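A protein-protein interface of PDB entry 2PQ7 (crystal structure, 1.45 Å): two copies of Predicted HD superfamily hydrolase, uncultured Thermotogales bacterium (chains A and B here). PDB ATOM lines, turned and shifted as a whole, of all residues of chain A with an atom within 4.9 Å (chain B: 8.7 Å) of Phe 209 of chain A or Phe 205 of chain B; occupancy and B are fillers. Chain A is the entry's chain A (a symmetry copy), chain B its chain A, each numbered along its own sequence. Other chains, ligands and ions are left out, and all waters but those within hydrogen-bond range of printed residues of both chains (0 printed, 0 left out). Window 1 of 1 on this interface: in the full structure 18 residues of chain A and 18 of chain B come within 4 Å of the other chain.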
ATOM      1  N   ILE A 142      25.531  28.211  21.744  1.00  0.00           N
ATOM      2  CA  ILE A 142      24.472  27.243  21.440  1.00  0.00           C
ATOM      3  C   ILE A 142      23.120  27.817  21.847  1.00  0.00           C
ATOM      4  O   ILE A 142      22.168  27.774  21.078  1.00  0.00           O
ATOM      5  CB  ILE A 142      24.704  25.884  22.137  1.00  0.00           C
ATOM      6  CG1 ILE A 142      25.909  25.152  21.549  1.00  0.00           C
ATOM      7  CG2 ILE A 142      23.453  25.002  22.033  1.00  0.00           C
ATOM      8  CD1 ILE A 142      26.461  24.047  22.464  1.00  0.00           C
ATOM      9  N   PHE A 146      19.602  28.858  19.355  1.00  0.00           N
ATOM     10  CA  PHE A 146      18.228  28.437  19.583  1.00  0.00           C
ATOM     11  C   PHE A 146      17.273  29.568  19.963  1.00  0.00           C
ATOM     12  O   PHE A 146      16.093  29.543  19.576  1.00  0.00           O
ATOM     13  CB  PHE A 146      18.198  27.238  20.544  1.00  0.00           C
ATOM     14  CG  PHE A 146      18.756  25.996  19.921  1.00  0.00           C
ATOM     15  CD1 PHE A 146      18.076  25.362  18.896  1.00  0.00           C
ATOM     16  CD2 PHE A 146      19.952  25.454  20.330  1.00  0.00           C
ATOM     17  CE1 PHE A 146      18.580  24.218  18.293  1.00  0.00           C
ATOM     18  CE2 PHE A 146      20.444  24.310  19.728  1.00  0.00           C
ATOM     19  CZ  PHE A 146      19.759  23.698  18.712  1.00  0.00           C
ATOM     20  N   PHE A 205      32.696  20.420  23.150  1.00  0.00           N
ATOM     21  CA  PHE A 205      31.391  20.457  23.802  1.00  0.00           C
ATOM     22  C   PHE A 205      30.298  20.695  22.765  1.00  0.00           C
ATOM     23  O   PHE A 205      29.243  20.023  22.796  1.00  0.00           O
ATOM     24  CB  PHE A 205      31.328  21.517  24.928  1.00  0.00           C
ATOM     25  CG  PHE A 205      30.010  21.533  25.642  1.00  0.00           C
ATOM     26  CD1 PHE A 205      29.707  20.514  26.502  1.00  0.00           C
ATOM     27  CD2 PHE A 205      29.057  22.485  25.366  1.00  0.00           C
ATOM     28  CE1 PHE A 205      28.491  20.474  27.157  1.00  0.00           C
ATOM     29  CE2 PHE A 205      27.807  22.444  26.030  1.00  0.00           C
ATOM     30  CZ  PHE A 205      27.546  21.427  26.896  1.00  0.00           C
ATOM     31  N   VAL A 206      30.536  21.606  21.838  1.00  0.00           N
ATOM     32  CA  VAL A 206      29.588  21.884  20.767  1.00  0.00           C
ATOM     33  C   VAL A 206      29.356  20.634  19.909  1.00  0.00           C
ATOM     34  O   VAL A 206      28.203  20.330  19.581  1.00  0.00           O
ATOM     35  CB  VAL A 206      30.009  23.092  19.913  1.00  0.00           C
ATOM     36  CG1 VAL A 206      29.070  23.271  18.719  1.00  0.00           C
ATOM     37  CG2 VAL A 206      30.045  24.359  20.762  1.00  0.00           C
ATOM     38  N   VAL A 207      30.421  19.905  19.587  1.00  0.00           N
ATOM     39  CA  VAL A 207      30.307  18.687  18.787  1.00  0.00           C
ATOM     40  C   VAL A 207      29.456  17.661  19.524  1.00  0.00           C
ATOM     41  O   VAL A 207      28.523  17.086  18.942  1.00  0.00           O
ATOM     42  CB  VAL A 207      31.693  18.116  18.396  1.00  0.00           C
ATOM     43  CG1 VAL A 207      31.562  16.712  17.824  1.00  0.00           C
ATOM     44  CG2 VAL A 207      32.394  19.067  17.422  1.00  0.00           C
ATOM     45  N   GLU A 208      29.755  17.438  20.799  1.00  0.00           N
ATOM     46  CA  GLU A 208      28.956  16.532  21.606  1.00  0.00           C
ATOM     47  C   GLU A 208      27.479  16.955  21.640  1.00  0.00           C
ATOM     48  O   GLU A 208      26.583  16.102  21.552  1.00  0.00           O
ATOM     49  CB  GLU A 208      29.474  16.437  23.026  1.00  0.00           C
ATOM     50  CG  GLU A 208      28.670  15.431  23.887  1.00  0.00           C
ATOM     51  CD  GLU A 208      29.239  15.222  25.258  1.00  0.00           C
ATOM     52  OE1 GLU A 208      30.383  15.666  25.515  1.00  0.00           O
ATOM     53  OE2 GLU A 208      28.553  14.637  26.110  1.00  0.00           O
ATOM     54  N   PHE A 209      27.214  18.249  21.774  1.00  0.00           N
ATOM     55  CA  PHE A 209      25.846  18.743  21.768  1.00  0.00           C
ATOM     56  C   PHE A 209      25.141  18.328  20.472  1.00  0.00           C
ATOM     57  O   PHE A 209      24.003  17.836  20.517  1.00  0.00           O
ATOM     58  CB  PHE A 209      25.770  20.265  21.917  1.00  0.00           C
ATOM     59  CG  PHE A 209      24.361  20.772  22.088  1.00  0.00           C
ATOM     60  CD1 PHE A 209      23.536  20.929  20.994  1.00  0.00           C
ATOM     61  CD2 PHE A 209      23.849  21.038  23.352  1.00  0.00           C
ATOM     62  CE1 PHE A 209      22.224  21.348  21.165  1.00  0.00           C
ATOM     63  CE2 PHE A 209      22.562  21.466  23.511  1.00  0.00           C
ATOM     64  CZ  PHE A 209      21.749  21.610  22.430  1.00  0.00           C
ATOM     65  N   VAL A 210      25.795  18.542  19.340  1.00  0.00           N
ATOM     66  CA  VAL A 210      25.220  18.219  18.032  1.00  0.00           C
ATOM     67  C   VAL A 210      24.995  16.720  17.885  1.00  0.00           C
ATOM     68  O   VAL A 210      23.952  16.279  17.415  1.00  0.00           O
ATOM     69  CB  VAL A 210      26.104  18.739  16.886  1.00  0.00           C
ATOM     70  CG1 VAL A 210      25.601  18.230  15.534  1.00  0.00           C
ATOM     71  CG2 VAL A 210      26.119  20.235  16.867  1.00  0.00           C
ATOM     72  N   GLN A 211      25.972  15.941  18.288  1.00  0.00           N
ATOM     73  CA  GLN A 211      25.864  14.508  18.201  1.00  0.00           C
ATOM     74  C   GLN A 211      24.683  14.024  19.009  1.00  0.00           C
ATOM     75  O   GLN A 211      23.908  13.184  18.521  1.00  0.00           O
ATOM     76  CB  GLN A 211      27.156  13.846  18.663  1.00  0.00           C
ATOM     77  CG  GLN A 211      28.304  14.059  17.689  1.00  0.00           C
ATOM     78  CD  GLN A 211      29.631  13.548  18.219  1.00  0.00           C
ATOM     79  OE1 GLN A 211      29.811  13.389  19.429  1.00  0.00           O
ATOM     80  NE2 GLN A 211      30.576  13.303  17.314  1.00  0.00           N
ATOM     81  N   ARG A 212      24.544  14.530  20.237  1.00  0.00           N
ATOM     82  CA  ARG A 212      23.451  14.158  21.107  1.00  0.00           C
ATOM     83  C   ARG A 212      22.114  14.592  20.546  1.00  0.00           C
ATOM     84  O   ARG A 212      21.164  13.832  20.596  1.00  0.00           O
ATOM     85  CB  ARG A 212      23.624  14.738  22.521  1.00  0.00           C
ATOM     86  CG  ARG A 212      24.687  14.066  23.341  1.00  0.00           C
ATOM     87  CD  ARG A 212      24.825  14.717  24.716  1.00  0.00           C
ATOM     88  NE  ARG A 212      25.819  13.990  25.471  1.00  0.00           N
ATOM     89  CZ  ARG A 212      25.572  12.895  26.174  1.00  0.00           C
ATOM     90  NH1 ARG A 212      24.344  12.376  26.228  1.00  0.00           N
ATOM     91  NH2 ARG A 212      26.575  12.279  26.799  1.00  0.00           N
ATOM     92  N   PHE A 213      22.039  15.818  20.042  1.00  0.00           N
ATOM     93  CA  PHE A 213      20.833  16.347  19.425  1.00  0.00           C
ATOM     94  C   PHE A 213      20.366  15.403  18.321  1.00  0.00           C
ATOM     95  O   PHE A 213      19.205  14.982  18.300  1.00  0.00           O
ATOM     96  CB  PHE A 213      21.091  17.749  18.854  1.00  0.00           C
ATOM     97  CG  PHE A 213      19.861  18.464  18.402  1.00  0.00           C
ATOM     98  CD1 PHE A 213      19.343  18.225  17.150  1.00  0.00           C
ATOM     99  CD2 PHE A 213      19.235  19.373  19.207  1.00  0.00           C
ATOM    100  CE1 PHE A 213      18.209  18.893  16.723  1.00  0.00           C
ATOM    101  CE2 PHE A 213      18.090  20.031  18.804  1.00  0.00           C
ATOM    102  CZ  PHE A 213      17.585  19.805  17.560  1.00  0.00           C
ATOM    103  N   ILE B 137      14.801  15.504  29.287  1.00  0.00           N
ATOM    104  CA  ILE B 137      16.212  15.820  29.453  1.00  0.00           C
ATOM    105  C   ILE B 137      17.082  15.510  28.264  1.00  0.00           C
ATOM    106  O   ILE B 137      16.783  14.671  27.429  1.00  0.00           O
ATOM    107  CB  ILE B 137      16.812  15.161  30.688  1.00  0.00           C
ATOM    108  CG1 ILE B 137      16.652  13.648  30.648  1.00  0.00           C
ATOM    109  CG2 ILE B 137      16.173  15.736  31.941  1.00  0.00           C
ATOM    110  CD1 ILE B 137      17.139  12.949  31.906  1.00  0.00           C
ATOM    111  N   GLY B 138      18.212  16.209  28.179  1.00  0.00           N
ATOM    112  CA  GLY B 138      19.125  16.000  27.081  1.00  0.00           C
ATOM    113  C   GLY B 138      19.305  17.242  26.217  1.00  0.00           C
ATOM    114  O   GLY B 138      18.788  18.321  26.541  1.00  0.00           O
ATOM    115  N   ALA B 139      19.998  17.063  25.106  1.00  0.00           N
ATOM    116  CA  ALA B 139      20.333  18.152  24.193  1.00  0.00           C
ATOM    117  C   ALA B 139      19.105  18.763  23.532  1.00  0.00           C
ATOM    118  O   ALA B 139      18.971  19.984  23.441  1.00  0.00           O
ATOM    119  CB  ALA B 139      21.289  17.672  23.153  1.00  0.00           C
ATOM    120  N   VAL B 140      18.163  17.937  23.078  1.00  0.00           N
ATOM    121  CA  VAL B 140      16.964  18.472  22.434  1.00  0.00           C
ATOM    122  C   VAL B 140      16.132  19.244  23.433  1.00  0.00           C
ATOM    123  O   VAL B 140      15.610  20.315  23.109  1.00  0.00           O
ATOM    124  CB  VAL B 140      16.125  17.369  21.717  1.00  0.00           C
ATOM    125  CG1 VAL B 140      14.851  17.959  21.140  1.00  0.00           C
ATOM    126  CG2 VAL B 140      16.935  16.706  20.612  1.00  0.00           C
ATOM    127  N   ALA B 141      16.006  18.727  24.659  1.00  0.00           N
ATOM    128  CA  ALA B 141      15.299  19.439  25.726  1.00  0.00           C
ATOM    129  C   ALA B 141      15.924  20.840  26.002  1.00  0.00           C
ATOM    130  O   ALA B 141      15.205  21.811  26.173  1.00  0.00           O
ATOM    131  CB  ALA B 141      15.287  18.597  26.995  1.00  0.00           C
ATOM    132  N   ILE B 142      17.250  20.895  26.064  1.00  0.00           N
ATOM    133  CA  ILE B 142      17.960  22.169  26.217  1.00  0.00           C
ATOM    134  C   ILE B 142      17.594  23.101  25.068  1.00  0.00           C
ATOM    135  O   ILE B 142      17.271  24.263  25.286  1.00  0.00           O
ATOM    136  CB  ILE B 142      19.491  21.982  26.283  1.00  0.00           C
ATOM    137  CG1 ILE B 142      19.915  21.286  27.575  1.00  0.00           C
ATOM    138  CG2 ILE B 142      20.208  23.333  26.155  1.00  0.00           C
ATOM    139  CD1 ILE B 142      21.324  20.672  27.506  1.00  0.00           C
ATOM    140  N   ALA B 143      17.699  22.619  23.837  1.00  0.00           N
ATOM    141  CA  ALA B 143      17.349  23.429  22.692  1.00  0.00           C
ATOM    142  C   ALA B 143      15.898  23.939  22.807  1.00  0.00           C
ATOM    143  O   ALA B 143      15.627  25.109  22.488  1.00  0.00           O
ATOM    144  CB  ALA B 143      17.567  22.688  21.402  1.00  0.00           C
ATOM    145  N   ARG B 144      14.967  23.092  23.281  1.00  0.00           N
ATOM    146  CA  ARG B 144      13.574  23.536  23.401  1.00  0.00           C
ATOM    147  C   ARG B 144      13.409  24.653  24.373  1.00  0.00           C
ATOM    148  O   ARG B 144      12.611  25.557  24.148  1.00  0.00           O
ATOM    149  CB  ARG B 144      12.626  22.412  23.869  1.00  0.00           C
ATOM    150  CG  ARG B 144      12.004  21.607  22.781  1.00  0.00           C
ATOM    151  CD  ARG B 144      10.702  20.898  23.312  1.00  0.00           C
ATOM    152  NE  ARG B 144      10.959  20.125  24.530  1.00  0.00           N
ATOM    153  CZ  ARG B 144      11.636  18.984  24.549  1.00  0.00           C
ATOM    154  NH1 ARG B 144      12.138  18.485  23.420  1.00  0.00           N
ATOM    155  NH2 ARG B 144      11.841  18.352  25.707  1.00  0.00           N
ATOM    156  N   PHE B 146      15.478  26.999  25.125  1.00  0.00           N
ATOM    157  CA  PHE B 146      15.926  28.233  24.497  1.00  0.00           C
ATOM    158  C   PHE B 146      15.058  28.700  23.329  1.00  0.00           C
ATOM    159  O   PHE B 146      14.882  29.914  23.131  1.00  0.00           O
ATOM    160  CB  PHE B 146      17.426  28.143  24.171  1.00  0.00           C
ATOM    161  CG  PHE B 146      18.276  28.151  25.402  1.00  0.00           C
ATOM    162  CD1 PHE B 146      18.376  29.293  26.177  1.00  0.00           C
ATOM    163  CD2 PHE B 146      18.970  27.035  25.811  1.00  0.00           C
ATOM    164  CE1 PHE B 146      19.147  29.320  27.331  1.00  0.00           C
ATOM    165  CE2 PHE B 146      19.741  27.072  26.958  1.00  0.00           C
ATOM    166  CZ  PHE B 146      19.825  28.211  27.715  1.00  0.00           C
ATOM    167  N   MET B 198      20.640   5.960  30.718  1.00  0.00           N
ATOM    168  CA  MET B 198      20.408   7.021  29.739  1.00  0.00           C
ATOM    169  C   MET B 198      20.076   8.335  30.426  1.00  0.00           C
ATOM    170  O   MET B 198      20.514   9.401  29.961  1.00  0.00           O
ATOM    171  CB  MET B 198      19.285   6.620  28.776  1.00  0.00           C
ATOM    172  CG  MET B 198      19.684   5.496  27.830  1.00  0.00           C
ATOM    173  SD  MET B 198      18.167   4.711  26.863  1.00  0.00           S
ATOM    174  CE  MET B 198      17.888   5.924  25.390  1.00  0.00           C
ATOM    175  N   ALA B 199      19.297   8.273  31.507  1.00  0.00           N
ATOM    176  CA  ALA B 199      18.915   9.436  32.275  1.00  0.00           C
ATOM    177  C   ALA B 199      20.153  10.035  32.953  1.00  0.00           C
ATOM    178  O   ALA B 199      20.343  11.254  32.932  1.00  0.00           O
ATOM    179  CB  ALA B 199      17.890   9.087  33.307  1.00  0.00           C
ATOM    180  N   GLU B 200      20.998   9.177  33.525  1.00  0.00           N
ATOM    181  CA  GLU B 200      22.224   9.647  34.162  1.00  0.00           C
ATOM    182  C   GLU B 200      23.126  10.367  33.161  1.00  0.00           C
ATOM    183  O   GLU B 200      23.681  11.429  33.442  1.00  0.00           O
ATOM    184  CB  GLU B 200      22.978   8.462  34.770  1.00  0.00           C
ATOM    185  CG  GLU B 200      24.268   8.834  35.475  1.00  0.00           C
ATOM    186  N   ASP B 201      23.267   9.787  31.986  1.00  0.00           N
ATOM    187  CA  ASP B 201      24.075  10.337  30.941  1.00  0.00           C
ATOM    188  C   ASP B 201      23.509  11.695  30.461  1.00  0.00           C
ATOM    189  O   ASP B 201      24.245  12.705  30.373  1.00  0.00           O
ATOM    190  CB  ASP B 201      24.100   9.331  29.822  1.00  0.00           C
ATOM    191  CG  ASP B 201      24.861   9.790  28.625  1.00  0.00           C
ATOM    192  OD1 ASP B 201      26.070  10.141  28.736  1.00  0.00           O
ATOM    193  OD2 ASP B 201      24.272   9.763  27.526  1.00  0.00           O
ATOM    194  N   ARG B 202      22.222  11.729  30.139  1.00  0.00           N
ATOM    195  CA  ARG B 202      21.615  12.981  29.712  1.00  0.00           C
ATOM    196  C   ARG B 202      21.659  14.050  30.794  1.00  0.00           C
ATOM    197  O   ARG B 202      21.930  15.217  30.482  1.00  0.00           O
ATOM    198  CB  ARG B 202      20.179  12.757  29.280  1.00  0.00           C
ATOM    199  CG  ARG B 202      20.103  11.993  28.005  1.00  0.00           C
ATOM    200  CD  ARG B 202      18.650  11.804  27.658  1.00  0.00           C
ATOM    201  NE  ARG B 202      18.485  11.036  26.437  1.00  0.00           N
ATOM    202  CZ  ARG B 202      17.376  11.026  25.706  1.00  0.00           C
ATOM    203  NH1 ARG B 202      16.349  11.790  26.029  1.00  0.00           N
ATOM    204  NH2 ARG B 202      17.342  10.341  24.575  1.00  0.00           N
ATOM    205  N   TYR B 203      21.387  13.695  32.044  1.00  0.00           N
ATOM    206  CA  TYR B 203      21.392  14.627  33.158  1.00  0.00           C
ATOM    207  C   TYR B 203      22.802  15.218  33.377  1.00  0.00           C
ATOM    208  O   TYR B 203      22.953  16.419  33.618  1.00  0.00           O
ATOM    209  CB  TYR B 203      20.898  13.904  34.406  1.00  0.00           C
ATOM    210  CG  TYR B 203      20.697  14.792  35.600  1.00  0.00           C
ATOM    211  CD1 TYR B 203      21.737  15.045  36.490  1.00  0.00           C
ATOM    212  CD2 TYR B 203      19.476  15.394  35.831  1.00  0.00           C
ATOM    213  CE1 TYR B 203      21.561  15.869  37.579  1.00  0.00           C
ATOM    214  CE2 TYR B 203      19.287  16.221  36.924  1.00  0.00           C
ATOM    215  CZ  TYR B 203      20.335  16.455  37.794  1.00  0.00           C
ATOM    216  OH  TYR B 203      20.148  17.286  38.884  1.00  0.00           O
ATOM    217  N   SER B 204      23.824  14.376  33.297  1.00  0.00           N
ATOM    218  CA  SER B 204      25.200  14.854  33.452  1.00  0.00           C
ATOM    219  C   SER B 204      25.603  15.792  32.297  1.00  0.00           C
ATOM    220  O   SER B 204      26.476  16.658  32.473  1.00  0.00           O
ATOM    221  CB  SER B 204      26.171  13.693  33.573  1.00  0.00           C
ATOM    222  OG  SER B 204      25.892  12.956  34.740  1.00  0.00           O
ATOM    223  N   PHE B 205      25.021  15.591  31.112  1.00  0.00           N
ATOM    224  CA  PHE B 205      25.247  16.501  29.994  1.00  0.00           C
ATOM    225  C   PHE B 205      24.550  17.832  30.258  1.00  0.00           C
ATOM    226  O   PHE B 205      25.142  18.910  30.027  1.00  0.00           O
ATOM    227  CB  PHE B 205      24.793  15.894  28.645  1.00  0.00           C
ATOM    228  CG  PHE B 205      25.064  16.796  27.478  1.00  0.00           C
ATOM    229  CD1 PHE B 205      26.351  16.952  27.044  1.00  0.00           C
ATOM    230  CD2 PHE B 205      24.066  17.554  26.912  1.00  0.00           C
ATOM    231  CE1 PHE B 205      26.648  17.797  25.992  1.00  0.00           C
ATOM    232  CE2 PHE B 205      24.368  18.426  25.837  1.00  0.00           C
ATOM    233  CZ  PHE B 205      25.657  18.542  25.416  1.00  0.00           C
ATOM    234  N   VAL B 206      23.329  17.783  30.759  1.00  0.00           N
ATOM    235  CA  VAL B 206      22.584  18.989  31.100  1.00  0.00           C
ATOM    236  C   VAL B 206      23.321  19.796  32.175  1.00  0.00           C
ATOM    237  O   VAL B 206      23.422  21.022  32.049  1.00  0.00           O
ATOM    238  CB  VAL B 206      21.134  18.684  31.509  1.00  0.00           C
ATOM    239  CG1 VAL B 206      20.423  19.950  31.989  1.00  0.00           C
ATOM    240  CG2 VAL B 206      20.373  18.051  30.347  1.00  0.00           C
ATOM    241  N   VAL B 207      23.857  19.122  33.190  1.00  0.00           N
ATOM    242  CA  VAL B 207      24.593  19.795  34.258  1.00  0.00           C
ATOM    243  C   VAL B 207      25.819  20.492  33.683  1.00  0.00           C
ATOM    244  O   VAL B 207      26.056  21.676  33.965  1.00  0.00           O
ATOM    245  CB  VAL B 207      24.963  18.825  35.408  1.00  0.00           C
ATOM    246  CG1 VAL B 207      25.966  19.464  36.357  1.00  0.00           C
ATOM    247  CG2 VAL B 207      23.696  18.371  36.137  1.00  0.00           C
ATOM    248  N   GLU B 208      26.589  19.777  32.870  1.00  0.00           N
ATOM    249  CA  GLU B 208      27.740  20.375  32.216  1.00  0.00           C
ATOM    250  C   GLU B 208      27.342  21.596  31.371  1.00  0.00           C
ATOM    251  O   GLU B 208      28.048  22.616  31.376  1.00  0.00           O
ATOM    252  CB  GLU B 208      28.465  19.380  31.332  1.00  0.00           C
ATOM    253  CG  GLU B 208      29.729  19.982  30.670  1.00  0.00           C
ATOM    254  CD  GLU B 208      30.536  18.985  29.894  1.00  0.00           C
ATOM    255  OE1 GLU B 208      30.277  17.765  30.019  1.00  0.00           O
ATOM    256  OE2 GLU B 208      31.421  19.396  29.128  1.00  0.00           O
ATOM    257  N   PHE B 209      26.235  21.504  30.645  1.00  0.00           N
ATOM    258  CA  PHE B 209      25.758  22.628  29.853  1.00  0.00           C
ATOM    259  C   PHE B 209      25.542  23.851  30.751  1.00  0.00           C
ATOM    260  O   PHE B 209      25.977  24.960  30.402  1.00  0.00           O
ATOM    261  CB  PHE B 209      24.457  22.313  29.109  1.00  0.00           C
ATOM    262  CG  PHE B 209      24.047  23.402  28.152  1.00  0.00           C
ATOM    263  CD1 PHE B 209      23.403  24.532  28.611  1.00  0.00           C
ATOM    264  CD2 PHE B 209      24.355  23.314  26.799  1.00  0.00           C
ATOM    265  CE1 PHE B 209      23.073  25.553  27.730  1.00  0.00           C
ATOM    266  CE2 PHE B 209      24.012  24.315  25.936  1.00  0.00           C
ATOM    267  CZ  PHE B 209      23.386  25.432  26.395  1.00  0.00           C
ATOM    268  N   VAL B 210      24.864  23.658  31.873  1.00  0.00           N
ATOM    269  CA  VAL B 210      24.562  24.749  32.802  1.00  0.00           C
ATOM    270  C   VAL B 210      25.837  25.328  33.402  1.00  0.00           C
ATOM    271  O   VAL B 210      26.000  26.540  33.492  1.00  0.00           O
ATOM    272  CB  VAL B 210      23.610  24.290  33.918  1.00  0.00           C
ATOM    273  CG1 VAL B 210      23.457  25.373  34.987  1.00  0.00           C
ATOM    274  CG2 VAL B 210      22.260  23.963  33.361  1.00  0.00           C
ATOM    275  N   GLN B 211      26.735  24.463  33.810  1.00  0.00           N
ATOM    276  CA  GLN B 211      27.980  24.900  34.388  1.00  0.00           C
ATOM    277  C   GLN B 211      28.744  25.749  33.399  1.00  0.00           C
ATOM    278  O   GLN B 211      29.264  26.813  33.778  1.00  0.00           O
ATOM    279  CB  GLN B 211      28.806  23.704  34.842  1.00  0.00           C
ATOM    280  CG  GLN B 211      28.212  23.006  36.054  1.00  0.00           C
ATOM    281  CD  GLN B 211      28.934  21.719  36.411  1.00  0.00           C
ATOM    282  OE1 GLN B 211      29.615  21.124  35.573  1.00  0.00           O
ATOM    283  NE2 GLN B 211      28.776  21.276  37.655  1.00  0.00           N
ATOM    284  N   ARG B 212      28.829  25.289  32.148  1.00  0.00           N
ATOM    285  CA  ARG B 212      29.523  26.012  31.106  1.00  0.00           C
ATOM    286  C   ARG B 212      28.855  27.335  30.801  1.00  0.00           C
ATOM    287  O   ARG B 212      29.537  28.331  30.635  1.00  0.00           O
ATOM    288  CB  ARG B 212      29.632  25.185  29.814  1.00  0.00           C
ATOM    289  CG  ARG B 212      30.622  24.057  29.880  1.00  0.00           C
ATOM    290  CD  ARG B 212      30.648  23.262  28.577  1.00  0.00           C
ATOM    291  NE  ARG B 212      31.656  22.233  28.687  1.00  0.00           N
ATOM    292  CZ  ARG B 212      32.944  22.417  28.434  1.00  0.00           C
ATOM    293  NH1 ARG B 212      33.405  23.608  28.048  1.00  0.00           N
ATOM    294  NH2 ARG B 212      33.795  21.407  28.610  1.00  0.00           N
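Phe 146 of chain B touches Phe 146 of chain A (O to O, 3.8 Å).
Phe 205 of chain A touches Phe 205 of chain B.
Glu 208 of chain B touches Phe 205 of chain A.
CE2 of Phe 205 of chain A touches CD2 of Phe 209 of chain B (3.6 Å).
Arg 212 of chain B touches Phe 205 of chain A.
OE2 of Glu 208 of chain A touches CD1 of Phe 205 of chain B, at 3.3 Å.
O of Ala 139 of chain B touches CZ of Phe 209 of chain A (3.4 Å).
CB of Ala 139 of chain B touches CB of Arg 212 of chain A (3.8 Å).
Phe 213 of chain A touches Ala 139 of chain B (N to CB, 3.7 Å).
Phe 213 of chain A touches Val 140 of chain B (O to CG2, 3.7 Å).
Printed residues of chain A that touch a printed residue of chain B: Phe 146, Phe 205, Glu 208, Phe 209, Arg 212 and Phe 213.
Hydrophobic or aromatic side chains of chain A within 4 Å of the printed part of chain B: Phe 146, Phe 205, Phe 209 and Phe 213.
Of the 24 printed residues of chain B, 9 touch a printed residue of chain A.
Printed residues of chain B that touch a printed residue of chain A: Ala 139, Val 140, Ala 143, Phe 146, Asp 201, Phe 205, Glu 208, Phe 209 and Arg 212.
Hydrophobic or aromatic side chains of chain B within 4 Å of the printed part of chain A: Ala 139, Val 140, Ala 143, Phe 146, Phe 205 and Phe 209.
Among the printed residues, 15 pairs touch across the chains.
Among the printed residues, Asp or Glu carboxylates within 4 Å of a Lys or Arg side-chain nitrogen of the other chain: Arg 212 of chain A with Asp 201 of chain B (2.9 Å).
Phe 146 of chain B touches its own counterpart, Phe 146 of chain A.
Phe 205 of chain A touches its own counterpart, Phe 205 of chain B.
Phe 205 of chain A touches Phe 209 of chain B, and with the chains exchanged Phe 209 of chain A touches Phe 205 of chain B.
Phe 205 of chain A touches Arg 212 of chain B, and with the chains exchanged Arg 212 of chain A touches Phe 205 of chain B.
10 positions are printed for both chains.
Of the 15 pairs that touch across the chains among the printed residues, 8 have their exchanged pair printed and touching as well.
The side-chain carboxylate (OE2) of Glu 208 of chain A is in salt-bridge range of the guanidinium group (NE) of Arg 212 of chain A (2.9 Å).
The guanidinium group (NE) of Arg 212 of chain B is in salt-bridge range of the side-chain carboxylate (OE2) of Glu 208 of chain B, 2.9 Å away.
Printed residues of chain B within 4 Å of Glu 208 of chain A: Phe 205 (3.3 Å).
Printed residues of chain B within 4 Å of Phe 209 of chain A: Ala 139 (3.4 Å) and Phe 205 (3.6 Å).
Gly 138 of chain B touches none of the printed residues of chain A.
Of the printed residues of chain A, Ala 139 of chain B touches Phe 209, Arg 212 and Phe 213.
Printed residues of chain A within 4 Å of Phe 146 of chain B: Phe 146 (3.8 Å).
Tyr 203 of chain B touches none of the printed residues of chain A.
OD2 of Asp 201 of chain B is in salt-bridge range of NH1 of Arg 212 of chain A (2.9 Å).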
